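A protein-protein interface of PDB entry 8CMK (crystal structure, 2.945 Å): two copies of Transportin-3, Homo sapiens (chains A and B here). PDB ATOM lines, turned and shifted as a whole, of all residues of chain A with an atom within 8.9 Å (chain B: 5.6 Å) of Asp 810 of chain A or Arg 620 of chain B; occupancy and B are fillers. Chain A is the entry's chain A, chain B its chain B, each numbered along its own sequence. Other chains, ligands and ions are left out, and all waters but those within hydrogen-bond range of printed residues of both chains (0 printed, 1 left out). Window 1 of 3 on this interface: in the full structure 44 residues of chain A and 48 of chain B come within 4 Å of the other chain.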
ATOM      1  N   VAL A 807      11.374  12.918 -23.589  1.00  0.00           N
ATOM      2  CA  VAL A 807      12.504  13.820 -23.318  1.00  0.00           C
ATOM      3  C   VAL A 807      12.505  14.342 -21.876  1.00  0.00           C
ATOM      4  O   VAL A 807      13.583  14.399 -21.278  1.00  0.00           O
ATOM      5  CB  VAL A 807      12.714  14.981 -24.323  1.00  0.00           C
ATOM      6  CG1 VAL A 807      12.804  14.461 -25.747  1.00  0.00           C
ATOM      7  CG2 VAL A 807      11.702  16.117 -24.204  1.00  0.00           C
ATOM      8  N   ALA A 808      11.355  14.780 -21.336  1.00  0.00           N
ATOM      9  CA  ALA A 808      11.215  15.066 -19.909  1.00  0.00           C
ATOM     10  C   ALA A 808      12.351  15.919 -19.325  1.00  0.00           C
ATOM     11  O   ALA A 808      12.959  15.525 -18.331  1.00  0.00           O
ATOM     12  CB  ALA A 808      11.130  13.749 -19.166  1.00  0.00           C
ATOM     13  N   ASN A 809      12.573  17.136 -19.841  1.00  0.00           N
ATOM     14  CA  ASN A 809      13.653  17.989 -19.353  1.00  0.00           C
ATOM     15  C   ASN A 809      13.311  18.600 -17.982  1.00  0.00           C
ATOM     16  O   ASN A 809      14.196  18.796 -17.144  1.00  0.00           O
ATOM     17  CB  ASN A 809      14.031  19.046 -20.402  1.00  0.00           C
ATOM     18  CG  ASN A 809      15.405  19.663 -20.196  1.00  0.00           C
ATOM     19  OD1 ASN A 809      16.167  19.257 -19.316  1.00  0.00           O
ATOM     20  ND2 ASN A 809      15.749  20.644 -21.016  1.00  0.00           N
ATOM     21  N   ASP A 810      12.028  18.910 -17.732  1.00  0.00           N
ATOM     22  CA  ASP A 810      11.582  19.360 -16.415  1.00  0.00           C
ATOM     23  C   ASP A 810      11.329  18.155 -15.500  1.00  0.00           C
ATOM     24  O   ASP A 810      10.300  17.492 -15.620  1.00  0.00           O
ATOM     25  CB  ASP A 810      10.329  20.232 -16.535  1.00  0.00           C
ATOM     26  CG  ASP A 810       9.841  20.847 -15.232  1.00  0.00           C
ATOM     27  OD1 ASP A 810      10.544  20.733 -14.214  1.00  0.00           O
ATOM     28  OD2 ASP A 810       8.762  21.459 -15.251  1.00  0.00           O
ATOM     29  N   HIS A 811      12.243  17.903 -14.548  1.00  0.00           N
ATOM     30  CA  HIS A 811      12.104  16.784 -13.625  1.00  0.00           C
ATOM     31  C   HIS A 811      11.040  17.025 -12.548  1.00  0.00           C
ATOM     32  O   HIS A 811      10.793  16.145 -11.731  1.00  0.00           O
ATOM     33  CB  HIS A 811      13.457  16.431 -12.995  1.00  0.00           C
ATOM     34  CG  HIS A 811      14.425  15.797 -13.944  1.00  0.00           C
ATOM     35  ND1 HIS A 811      14.168  14.648 -14.665  1.00  0.00           N
ATOM     36  CD2 HIS A 811      15.667  16.175 -14.279  1.00  0.00           C
ATOM     37  CE1 HIS A 811      15.228  14.354 -15.407  1.00  0.00           C
ATOM     38  NE2 HIS A 811      16.151  15.270 -15.192  1.00  0.00           N
ATOM     39  N   GLU A 812      10.374  18.184 -12.555  1.00  0.00           N
ATOM     40  CA  GLU A 812       9.307  18.478 -11.605  1.00  0.00           C
ATOM     41  C   GLU A 812       7.934  18.036 -12.129  1.00  0.00           C
ATOM     42  O   GLU A 812       6.966  18.090 -11.381  1.00  0.00           O
ATOM     43  CB  GLU A 812       9.286  19.976 -11.314  1.00  0.00           C
ATOM     44  CG  GLU A 812       8.697  20.306  -9.963  1.00  0.00           C
ATOM     45  CD  GLU A 812       8.216  21.740  -9.820  1.00  0.00           C
ATOM     46  OE1 GLU A 812       7.224  22.111 -10.487  1.00  0.00           O
ATOM     47  OE2 GLU A 812       8.826  22.489  -9.033  1.00  0.00           O
ATOM     48  N   GLU A 813       7.828  17.597 -13.399  1.00  0.00           N
ATOM     49  CA  GLU A 813       6.568  17.143 -13.999  1.00  0.00           C
ATOM     50  C   GLU A 813       6.292  15.659 -13.695  1.00  0.00           C
ATOM     51  O   GLU A 813       7.176  14.917 -13.273  1.00  0.00           O
ATOM     52  CB  GLU A 813       6.613  17.421 -15.510  1.00  0.00           C
ATOM     53  CG  GLU A 813       5.299  17.242 -16.282  1.00  0.00           C
ATOM     54  CD  GLU A 813       4.027  17.858 -15.700  1.00  0.00           C
ATOM     55  OE1 GLU A 813       4.101  18.949 -15.107  1.00  0.00           O
ATOM     56  OE2 GLU A 813       2.945  17.258 -15.868  1.00  0.00           O
ATOM     57  N   ASP A 814       5.044  15.211 -13.919  1.00  0.00           N
ATOM     58  CA  ASP A 814       4.660  13.807 -13.820  1.00  0.00           C
ATOM     59  C   ASP A 814       5.127  13.016 -15.054  1.00  0.00           C
ATOM     60  O   ASP A 814       4.315  12.461 -15.792  1.00  0.00           O
ATOM     61  CB  ASP A 814       3.144  13.719 -13.606  1.00  0.00           C
ATOM     62  CG  ASP A 814       2.622  12.371 -13.130  1.00  0.00           C
ATOM     63  OD1 ASP A 814       3.452  11.479 -12.829  1.00  0.00           O
ATOM     64  OD2 ASP A 814       1.383  12.228 -13.064  1.00  0.00           O
ATOM     65  N   PHE A 815       6.451  12.891 -15.235  1.00  0.00           N
ATOM     66  CA  PHE A 815       7.046  12.334 -16.445  1.00  0.00           C
ATOM     67  C   PHE A 815       7.372  10.838 -16.332  1.00  0.00           C
ATOM     68  O   PHE A 815       7.532  10.176 -17.355  1.00  0.00           O
ATOM     69  CB  PHE A 815       8.319  13.113 -16.817  1.00  0.00           C
ATOM     70  CG  PHE A 815       9.548  12.808 -15.984  1.00  0.00           C
ATOM     71  CD1 PHE A 815      10.340  11.703 -16.271  1.00  0.00           C
ATOM     72  CD2 PHE A 815       9.912  13.603 -14.900  1.00  0.00           C
ATOM     73  CE1 PHE A 815      11.439  11.392 -15.479  1.00  0.00           C
ATOM     74  CE2 PHE A 815      11.013  13.289 -14.116  1.00  0.00           C
ATOM     75  CZ  PHE A 815      11.777  12.185 -14.405  1.00  0.00           C
ATOM     76  N   GLU A 816       7.503  10.291 -15.118  1.00  0.00           N
ATOM     77  CA  GLU A 816       8.182   9.014 -14.930  1.00  0.00           C
ATOM     78  C   GLU A 816       7.451   7.851 -15.611  1.00  0.00           C
ATOM     79  O   GLU A 816       8.110   6.948 -16.136  1.00  0.00           O
ATOM     80  CB  GLU A 816       8.392   8.727 -13.442  1.00  0.00           C
ATOM     81  CG  GLU A 816       9.436   9.619 -12.786  1.00  0.00           C
ATOM     82  CD  GLU A 816       8.955  10.926 -12.168  1.00  0.00           C
ATOM     83  OE1 GLU A 816       7.853  11.406 -12.520  1.00  0.00           O
ATOM     84  OE2 GLU A 816       9.669  11.440 -11.280  1.00  0.00           O
ATOM     85  N   ARG A 818       5.233   8.120 -18.311  1.00  0.00           N
ATOM     86  CA  ARG A 818       5.469   8.341 -19.736  1.00  0.00           C
ATOM     87  C   ARG A 818       6.826   7.771 -20.141  1.00  0.00           C
ATOM     88  O   ARG A 818       6.880   6.851 -20.940  1.00  0.00           O
ATOM     89  CB  ARG A 818       5.471   9.821 -20.127  1.00  0.00           C
ATOM     90  CG  ARG A 818       4.112  10.395 -20.497  1.00  0.00           C
ATOM     91  CD  ARG A 818       4.272  11.767 -21.150  1.00  0.00           C
ATOM     92  NE  ARG A 818       4.677  12.814 -20.218  1.00  0.00           N
ATOM     93  CZ  ARG A 818       5.859  13.432 -20.186  1.00  0.00           C
ATOM     94  NH1 ARG A 818       5.994  14.508 -19.432  1.00  0.00           N
ATOM     95  NH2 ARG A 818       6.878  13.036 -20.928  1.00  0.00           N
ATOM     96  N   LYS A 819       7.902   8.317 -19.569  1.00  0.00           N
ATOM     97  CA  LYS A 819       9.285   7.996 -19.895  1.00  0.00           C
ATOM     98  C   LYS A 819       9.488   6.488 -19.992  1.00  0.00           C
ATOM     99  O   LYS A 819      10.112   6.002 -20.935  1.00  0.00           O
ATOM    100  CB  LYS A 819      10.155   8.619 -18.798  1.00  0.00           C
ATOM    101  CG  LYS A 819      11.663   8.507 -18.968  1.00  0.00           C
ATOM    102  CD  LYS A 819      12.234   9.472 -19.974  1.00  0.00           C
ATOM    103  CE  LYS A 819      13.730   9.666 -19.848  1.00  0.00           C
ATOM    104  NZ  LYS A 819      14.066  10.507 -18.673  1.00  0.00           N
ATOM    105  N   LEU B 615       5.578  24.223  -2.277  1.00  0.00           N
ATOM    106  CA  LEU B 615       4.175  24.536  -2.528  1.00  0.00           C
ATOM    107  C   LEU B 615       3.844  24.411  -4.013  1.00  0.00           C
ATOM    108  O   LEU B 615       2.798  23.869  -4.350  1.00  0.00           O
ATOM    109  CB  LEU B 615       3.860  25.946  -2.032  1.00  0.00           C
ATOM    110  CG  LEU B 615       3.746  26.085  -0.518  1.00  0.00           C
ATOM    111  CD1 LEU B 615       3.794  27.544  -0.110  1.00  0.00           C
ATOM    112  CD2 LEU B 615       2.466  25.436  -0.002  1.00  0.00           C
ATOM    113  N   ALA B 616       4.755  24.867  -4.890  1.00  0.00           N
ATOM    114  CA  ALA B 616       4.622  24.729  -6.332  1.00  0.00           C
ATOM    115  C   ALA B 616       4.476  23.264  -6.761  1.00  0.00           C
ATOM    116  O   ALA B 616       3.558  22.948  -7.508  1.00  0.00           O
ATOM    117  CB  ALA B 616       5.794  25.406  -6.987  1.00  0.00           C
ATOM    118  N   VAL B 617       5.315  22.341  -6.268  1.00  0.00           N
ATOM    119  CA  VAL B 617       5.151  20.919  -6.568  1.00  0.00           C
ATOM    120  C   VAL B 617       3.771  20.430  -6.137  1.00  0.00           C
ATOM    121  O   VAL B 617       3.154  19.630  -6.840  1.00  0.00           O
ATOM    122  CB  VAL B 617       6.240  20.046  -5.911  1.00  0.00           C
ATOM    123  CG1 VAL B 617       5.948  18.546  -6.006  1.00  0.00           C
ATOM    124  CG2 VAL B 617       7.608  20.336  -6.500  1.00  0.00           C
ATOM    125  N   ILE B 618       3.300  20.887  -4.971  1.00  0.00           N
ATOM    126  CA  ILE B 618       2.031  20.430  -4.421  1.00  0.00           C
ATOM    127  C   ILE B 618       0.886  20.941  -5.293  1.00  0.00           C
ATOM    128  O   ILE B 618       0.011  20.163  -5.642  1.00  0.00           O
ATOM    129  CB  ILE B 618       1.870  20.831  -2.937  1.00  0.00           C
ATOM    130  CG1 ILE B 618       2.891  20.119  -2.043  1.00  0.00           C
ATOM    131  CG2 ILE B 618       0.440  20.597  -2.452  1.00  0.00           C
ATOM    132  CD1 ILE B 618       3.123  20.802  -0.715  1.00  0.00           C
ATOM    133  N   PHE B 619       0.907  22.221  -5.683  1.00  0.00           N
ATOM    134  CA  PHE B 619      -0.176  22.811  -6.456  1.00  0.00           C
ATOM    135  C   PHE B 619      -0.162  22.311  -7.900  1.00  0.00           C
ATOM    136  O   PHE B 619      -1.217  22.132  -8.497  1.00  0.00           O
ATOM    137  CB  PHE B 619      -0.072  24.336  -6.465  1.00  0.00           C
ATOM    138  CG  PHE B 619      -0.148  25.037  -5.134  1.00  0.00           C
ATOM    139  CD1 PHE B 619      -0.976  24.581  -4.121  1.00  0.00           C
ATOM    140  CD2 PHE B 619       0.556  26.211  -4.933  1.00  0.00           C
ATOM    141  CE1 PHE B 619      -1.055  25.258  -2.915  1.00  0.00           C
ATOM    142  CE2 PHE B 619       0.471  26.889  -3.730  1.00  0.00           C
ATOM    143  CZ  PHE B 619      -0.329  26.409  -2.720  1.00  0.00           C
ATOM    144  N   ARG B 620       1.029  22.056  -8.443  1.00  0.00           N
ATOM    145  CA  ARG B 620       1.190  21.514  -9.782  1.00  0.00           C
ATOM    146  C   ARG B 620       0.466  20.177  -9.953  1.00  0.00           C
ATOM    147  O   ARG B 620      -0.088  19.935 -11.022  1.00  0.00           O
ATOM    148  CB  ARG B 620       2.687  21.384 -10.068  1.00  0.00           C
ATOM    149  CG  ARG B 620       3.015  20.919 -11.476  1.00  0.00           C
ATOM    150  CD  ARG B 620       4.499  21.028 -11.748  1.00  0.00           C
ATOM    151  NE  ARG B 620       4.776  20.767 -13.154  1.00  0.00           N
ATOM    152  CZ  ARG B 620       5.815  21.251 -13.827  1.00  0.00           C
ATOM    153  NH1 ARG B 620       5.837  21.172 -15.142  1.00  0.00           N
ATOM    154  NH2 ARG B 620       6.794  21.882 -13.202  1.00  0.00           N
ATOM    155  N   HIS B 621       0.492  19.308  -8.927  1.00  0.00           N
ATOM    156  CA  HIS B 621      -0.001  17.940  -9.039  1.00  0.00           C
ATOM    157  C   HIS B 621      -1.345  17.697  -8.355  1.00  0.00           C
ATOM    158  O   HIS B 621      -1.988  16.697  -8.642  1.00  0.00           O
ATOM    159  CB  HIS B 621       1.066  16.979  -8.518  1.00  0.00           C
ATOM    160  CG  HIS B 621       2.292  17.105  -9.354  1.00  0.00           C
ATOM    161  ND1 HIS B 621       3.403  17.817  -8.959  1.00  0.00           N
ATOM    162  CD2 HIS B 621       2.517  16.720 -10.618  1.00  0.00           C
ATOM    163  CE1 HIS B 621       4.272  17.831  -9.957  1.00  0.00           C
ATOM    164  NE2 HIS B 621       3.766  17.150 -10.967  1.00  0.00           N
ATOM    165  N   THR B 622      -1.786  18.584  -7.464  1.00  0.00           N
ATOM    166  CA  THR B 622      -3.094  18.425  -6.847  1.00  0.00           C
ATOM    167  C   THR B 622      -4.169  18.954  -7.793  1.00  0.00           C
ATOM    168  O   THR B 622      -4.592  20.106  -7.685  1.00  0.00           O
ATOM    169  CB  THR B 622      -3.175  19.115  -5.483  1.00  0.00           C
ATOM    170  OG1 THR B 622      -2.088  18.644  -4.684  1.00  0.00           O
ATOM    171  CG2 THR B 622      -4.488  18.854  -4.781  1.00  0.00           C
ATOM    172  N   ASN B 623      -4.599  18.099  -8.732  1.00  0.00           N
ATOM    173  CA  ASN B 623      -5.586  18.471  -9.739  1.00  0.00           C
ATOM    174  C   ASN B 623      -6.736  17.462  -9.700  1.00  0.00           C
ATOM    175  O   ASN B 623      -6.844  16.604 -10.573  1.00  0.00           O
ATOM    176  CB  ASN B 623      -4.967  18.571 -11.142  1.00  0.00           C
ATOM    177  CG  ASN B 623      -3.615  19.257 -11.188  1.00  0.00           C
ATOM    178  OD1 ASN B 623      -2.670  18.749 -11.787  1.00  0.00           O
ATOM    179  ND2 ASN B 623      -3.519  20.423 -10.579  1.00  0.00           N
ATOM    180  N   ARG B 664       5.989  31.437 -10.272  1.00  0.00           N
ATOM    181  CA  ARG B 664       5.780  30.030 -10.542  1.00  0.00           C
ATOM    182  C   ARG B 664       4.920  29.350  -9.465  1.00  0.00           C
ATOM    183  O   ARG B 664       4.117  28.486  -9.780  1.00  0.00           O
ATOM    184  CB  ARG B 664       7.145  29.370 -10.665  1.00  0.00           C
ATOM    185  CG  ARG B 664       7.076  28.096 -11.474  1.00  0.00           C
ATOM    186  CD  ARG B 664       8.431  27.443 -11.542  1.00  0.00           C
ATOM    187  NE  ARG B 664       8.768  26.863 -10.255  1.00  0.00           N
ATOM    188  CZ  ARG B 664       8.672  25.571  -9.969  1.00  0.00           C
ATOM    189  NH1 ARG B 664       8.933  25.161  -8.743  1.00  0.00           N
ATOM    190  NH2 ARG B 664       8.292  24.697 -10.889  1.00  0.00           N
ATOM    191  N   PHE B 668       0.753  27.961 -10.344  1.00  0.00           N
ATOM    192  CA  PHE B 668       0.184  26.659 -10.078  1.00  0.00           C
ATOM    193  C   PHE B 668      -0.919  26.751  -9.027  1.00  0.00           C
ATOM    194  O   PHE B 668      -1.848  25.966  -9.083  1.00  0.00           O
ATOM    195  CB  PHE B 668       1.279  25.686  -9.666  1.00  0.00           C
ATOM    196  CG  PHE B 668       2.247  25.308 -10.759  1.00  0.00           C
ATOM    197  CD1 PHE B 668       1.802  24.744 -11.937  1.00  0.00           C
ATOM    198  CD2 PHE B 668       3.615  25.462 -10.593  1.00  0.00           C
ATOM    199  CE1 PHE B 668       2.699  24.373 -12.927  1.00  0.00           C
ATOM    200  CE2 PHE B 668       4.515  25.080 -11.577  1.00  0.00           C
ATOM    201  CZ  PHE B 668       4.054  24.539 -12.743  1.00  0.00           C
ATOM    202  N   ARG B 671      -3.980  27.463 -11.016  1.00  0.00           N
ATOM    203  CA  ARG B 671      -4.344  26.278 -11.794  1.00  0.00           C
ATOM    204  C   ARG B 671      -4.939  25.168 -10.906  1.00  0.00           C
ATOM    205  O   ARG B 671      -5.804  24.409 -11.341  1.00  0.00           O
ATOM    206  CB  ARG B 671      -3.143  25.781 -12.622  1.00  0.00           C
ATOM    207  CG  ARG B 671      -3.408  24.458 -13.328  1.00  0.00           C
ATOM    208  CD  ARG B 671      -2.557  24.116 -14.522  1.00  0.00           C
ATOM    209  NE  ARG B 671      -1.234  23.536 -14.308  1.00  0.00           N
ATOM    210  CZ  ARG B 671      -0.948  22.331 -13.827  1.00  0.00           C
ATOM    211  NH1 ARG B 671       0.199  21.759 -14.155  1.00  0.00           N
ATOM    212  NH2 ARG B 671      -1.820  21.666 -13.088  1.00  0.00           N
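No position is printed for both chains.
Of the 7 pairs that touch across the chains among the printed residues, none has its exchanged pair printed and touching as well.
Hydrophobic or aromatic side chains of chain B within 4 Å of the printed part of chain A: Val 617 and His 621.
Among the printed residues, Asp or Glu carboxylates within 4 Å of a Lys or Arg side-chain nitrogen of the other chain: Asp 810 of chain A with Arg 620 of chain B, Glu 812 of chain A with Arg 620 of chain B, Glu 812 of chain A with Arg 664 of chain B and Glu 813 of chain A with Arg 620 of chain B.
N of Glu 812 of chain A lies within hydrogen-bond range of OD1 of Asp 810 of chain A, at 3.0 Å.
The backbone carbonyl oxygen of Arg 620 of chain B lies close to the side-chain amide oxygen of Asn 623 of chain B (2.9 Å).
NH2 of Arg 671 of chain B is in hydrogen-bond range of O of Arg 620 of chain B.
ND1 of His 621 of chain B is in hydrogen-bond range of O of Val 617 of chain B (2.8 Å).
Among the printed residues, pairs that only touch across the chains: Glu 812 of chain A with Val 617 of chain B and Asp 814 of chain A with His 621 of chain B.
OE2 of Glu 812 of chain A is in salt-bridge range of NH1 of Arg 664 of chain B, 2.7 Å away.
A ring nitrogen (NE2) of His 621 of chain B lies close to the backbone carbonyl oxygen (O) of Glu 812 of chain A, at 3.4 Å.
NH2 of Arg 620 of chain B is in salt-bridge range of OE1 of Glu 812 of chain A (2.8 Å).
The side-chain carboxylate (OE1) of Glu 813 of chain A lies within salt-bridge range of the guanidinium group (NE) of Arg 620 of chain B.
OD2 of Asp 810 of chain A is in salt-bridge range of NH2 of Arg 620 of chain B, at 2.9 Å.
Asp 810 of chain A touches just one residue of chain B: Arg 620.
Of the printed residues of chain B, Glu 812 of chain A touches Val 617 (3.5 Å), Arg 620 (2.8 Å), His 621 (3.1 Å) and Arg 664 (2.7 Å).
Of chain A, only Asp 810 (2.9 Å), Glu 812 (2.8 Å) and Glu 813 (2.8 Å) come within 4 Å of Arg 620 of chain B.
Printed residues of chain A within 4 Å of Arg 664 of chain B: Glu 812 (2.7 Å).
The nearest residue of chain B that does not touch Asp 810 of chain A is Arg 664 of chain B (5.5 Å).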
